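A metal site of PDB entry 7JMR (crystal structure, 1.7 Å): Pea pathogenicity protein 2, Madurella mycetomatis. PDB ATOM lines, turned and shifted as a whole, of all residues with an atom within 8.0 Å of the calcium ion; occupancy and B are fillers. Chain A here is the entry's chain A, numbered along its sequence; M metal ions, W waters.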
ATOM      1  N   ARG A 223      -2.336   9.836 -15.924  1.00  0.00           N
ATOM      2  CA  ARG A 223      -1.754  10.680 -14.877  1.00  0.00           C
ATOM      3  C   ARG A 223      -0.502  11.391 -15.369  1.00  0.00           C
ATOM      4  O   ARG A 223      -0.296  12.583 -15.088  1.00  0.00           O
ATOM      5  CB  ARG A 223      -1.450   9.823 -13.639  1.00  0.00           C
ATOM      6  CG  ARG A 223      -0.763  10.589 -12.506  1.00  0.00           C
ATOM      7  CD  ARG A 223      -1.701  11.648 -11.898  1.00  0.00           C
ATOM      8  NE  ARG A 223      -1.043  12.255 -10.749  1.00  0.00           N
ATOM      9  CZ  ARG A 223      -1.022  11.750  -9.517  1.00  0.00           C
ATOM     10  NH1 ARG A 223      -1.626  10.598  -9.241  1.00  0.00           N
ATOM     11  NH2 ARG A 223      -0.367  12.364  -8.573  1.00  0.00           N
ATOM     12  N   GLU A 227       0.124  15.423 -15.425  1.00  0.00           N
ATOM     13  CA  GLU A 227       1.203  16.153 -14.767  1.00  0.00           C
ATOM     14  C   GLU A 227       2.046  16.907 -15.786  1.00  0.00           C
ATOM     15  O   GLU A 227       2.521  18.009 -15.491  1.00  0.00           O
ATOM     16  CB  GLU A 227       2.050  15.197 -13.943  1.00  0.00           C
ATOM     17  CG  GLU A 227       1.303  14.465 -12.836  1.00  0.00           C
ATOM     18  CD  GLU A 227       0.544  15.408 -11.891  1.00  0.00           C
ATOM     19  OE1 GLU A 227       0.928  16.584 -11.750  1.00  0.00           O
ATOM     20  OE2 GLU A 227      -0.429  14.954 -11.274  1.00  0.00           O
ATOM     21  N   VAL A 237       3.681  20.124  -9.809  1.00  0.00           N
ATOM     22  CA  VAL A 237       3.200  18.841 -10.267  1.00  0.00           C
ATOM     23  C   VAL A 237       3.289  17.888  -9.093  1.00  0.00           C
ATOM     24  O   VAL A 237       3.967  18.154  -8.100  1.00  0.00           O
ATOM     25  CB  VAL A 237       3.983  18.352 -11.484  1.00  0.00           C
ATOM     26  CG1 VAL A 237       3.756  19.342 -12.625  1.00  0.00           C
ATOM     27  CG2 VAL A 237       5.431  18.244 -11.138  1.00  0.00           C
ATOM     28  N   ASP A 238       2.630  16.744  -9.225  1.00  0.00           N
ATOM     29  CA  ASP A 238       2.692  15.679  -8.252  1.00  0.00           C
ATOM     30  C   ASP A 238       3.071  14.403  -9.010  1.00  0.00           C
ATOM     31  O   ASP A 238       2.206  13.722  -9.550  1.00  0.00           O
ATOM     32  CB  ASP A 238       1.368  15.529  -7.507  1.00  0.00           C
ATOM     33  CG  ASP A 238       1.392  14.408  -6.497  1.00  0.00           C
ATOM     34  OD1 ASP A 238       2.403  13.711  -6.404  1.00  0.00           O
ATOM     35  OD2 ASP A 238       0.386  14.264  -5.765  1.00  0.00           O
ATOM     36  N   LEU A 239       4.371  14.128  -9.036  1.00  0.00           N
ATOM     37  CA  LEU A 239       4.923  12.915  -9.624  1.00  0.00           C
ATOM     38  C   LEU A 239       5.247  11.865  -8.573  1.00  0.00           C
ATOM     39  O   LEU A 239       5.749  10.779  -8.924  1.00  0.00           O
ATOM     40  CB  LEU A 239       6.181  13.275 -10.416  1.00  0.00           C
ATOM     41  CG  LEU A 239       5.870  14.081 -11.682  1.00  0.00           C
ATOM     42  CD1 LEU A 239       7.201  14.583 -12.247  1.00  0.00           C
ATOM     43  CD2 LEU A 239       5.093  13.326 -12.710  1.00  0.00           C
ATOM     44  N   PHE A 240       4.938  12.137  -7.314  1.00  0.00           N
ATOM     45  CA  PHE A 240       5.224  11.212  -6.207  1.00  0.00           C
ATOM     46  C   PHE A 240       3.961  10.404  -5.996  1.00  0.00           C
ATOM     47  O   PHE A 240       2.977  10.900  -5.448  1.00  0.00           O
ATOM     48  CB  PHE A 240       5.648  12.004  -4.972  1.00  0.00           C
ATOM     49  CG  PHE A 240       6.980  12.702  -5.132  1.00  0.00           C
ATOM     50  CD1 PHE A 240       8.155  12.062  -4.820  1.00  0.00           C
ATOM     51  CD2 PHE A 240       7.036  14.004  -5.611  1.00  0.00           C
ATOM     52  CE1 PHE A 240       9.389  12.696  -4.953  1.00  0.00           C
ATOM     53  CE2 PHE A 240       8.270  14.637  -5.744  1.00  0.00           C
ATOM     54  CZ  PHE A 240       9.442  13.988  -5.421  1.00  0.00           C
ATOM     55  N   TRP A 241       3.942   9.162  -6.473  1.00  0.00           N
ATOM     56  CA  TRP A 241       2.688   8.451  -6.624  1.00  0.00           C
ATOM     57  C   TRP A 241       2.471   7.383  -5.569  1.00  0.00           C
ATOM     58  O   TRP A 241       1.511   6.623  -5.672  1.00  0.00           O
ATOM     59  CB  TRP A 241       2.586   7.856  -8.027  1.00  0.00           C
ATOM     60  CG  TRP A 241       2.491   8.905  -9.097  1.00  0.00           C
ATOM     61  CD1 TRP A 241       2.193  10.242  -8.930  1.00  0.00           C
ATOM     62  CD2 TRP A 241       2.736   8.727 -10.497  1.00  0.00           C
ATOM     63  NE1 TRP A 241       2.204  10.897 -10.146  1.00  0.00           N
ATOM     64  CE2 TRP A 241       2.553   9.989 -11.119  1.00  0.00           C
ATOM     65  CE3 TRP A 241       3.086   7.620 -11.292  1.00  0.00           C
ATOM     66  CZ2 TRP A 241       2.694  10.167 -12.502  1.00  0.00           C
ATOM     67  CZ3 TRP A 241       3.234   7.809 -12.655  1.00  0.00           C
ATOM     68  CH2 TRP A 241       3.045   9.063 -13.247  1.00  0.00           C
ATOM     69  N   GLU A 242       3.329   7.321  -4.561  1.00  0.00           N
ATOM     70  CA  GLU A 242       3.125   6.407  -3.443  1.00  0.00           C
ATOM     71  C   GLU A 242       2.537   7.090  -2.203  1.00  0.00           C
ATOM     72  O   GLU A 242       2.176   6.383  -1.252  1.00  0.00           O
ATOM     73  CB  GLU A 242       4.447   5.736  -3.051  1.00  0.00           C
ATOM     74  CG  GLU A 242       5.269   5.306  -4.255  1.00  0.00           C
ATOM     75  CD  GLU A 242       5.761   3.878  -4.166  1.00  0.00           C
ATOM     76  OE1 GLU A 242       5.954   3.359  -3.044  1.00  0.00           O
ATOM     77  OE2 GLU A 242       5.955   3.260  -5.249  1.00  0.00           O
ATOM     78  N   HIS A 243       2.481   8.417  -2.185  1.00  0.00           N
ATOM     79  CA  HIS A 243       1.911   9.212  -1.082  1.00  0.00           C
ATOM     80  C   HIS A 243       1.341  10.480  -1.704  1.00  0.00           C
ATOM     81  O   HIS A 243       1.718  10.783  -2.859  1.00  0.00           O
ATOM     82  CB  HIS A 243       2.960   9.555  -0.046  1.00  0.00           C
ATOM     83  CG  HIS A 243       3.568   8.348   0.599  1.00  0.00           C
ATOM     84  ND1 HIS A 243       4.725   7.770   0.140  1.00  0.00           N
ATOM     85  CD2 HIS A 243       3.140   7.577   1.625  1.00  0.00           C
ATOM     86  CE1 HIS A 243       5.005   6.702   0.878  1.00  0.00           C
ATOM     87  NE2 HIS A 243       4.058   6.567   1.783  1.00  0.00           N
HETATM   88 CA    CA M   1       1.437  12.343  -4.549  1.00  0.00          CA
HETATM   89  O   HOH W   1      -0.402  12.767  -2.971  1.00  0.00           O
HETATM   90  O   HOH W   2       2.775  13.837  -3.195  1.00  0.00           O
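The calcium ion is bound by O of Phe 240 (2.3 Å), O of His 243 (2.3 Å), water W2 (2.4 Å), water W1 (2.5 Å), OD1 of Asp 238 (2.5 Å) and OD2 of Asp 238 (2.5 Å). The calcium ion has six donor atoms within binding distance.
Of the 9 residues printed, 3 come within 4 Å of the calcium ion. The nearest printed residue that does not touch the calcium ion is Arg 223 (4.4 Å).
O of Asp 238 lies within hydrogen-bond range of NH2 of Arg 223 (3.1 Å). The indole nitrogen (NE1) of Trp 241 is in hydrogen-bond range of the backbone carbonyl oxygen (O) of Asp 238. OE1 of Glu 227 lies within hydrogen-bond range of N of Asp 238, at 3.0 Å.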
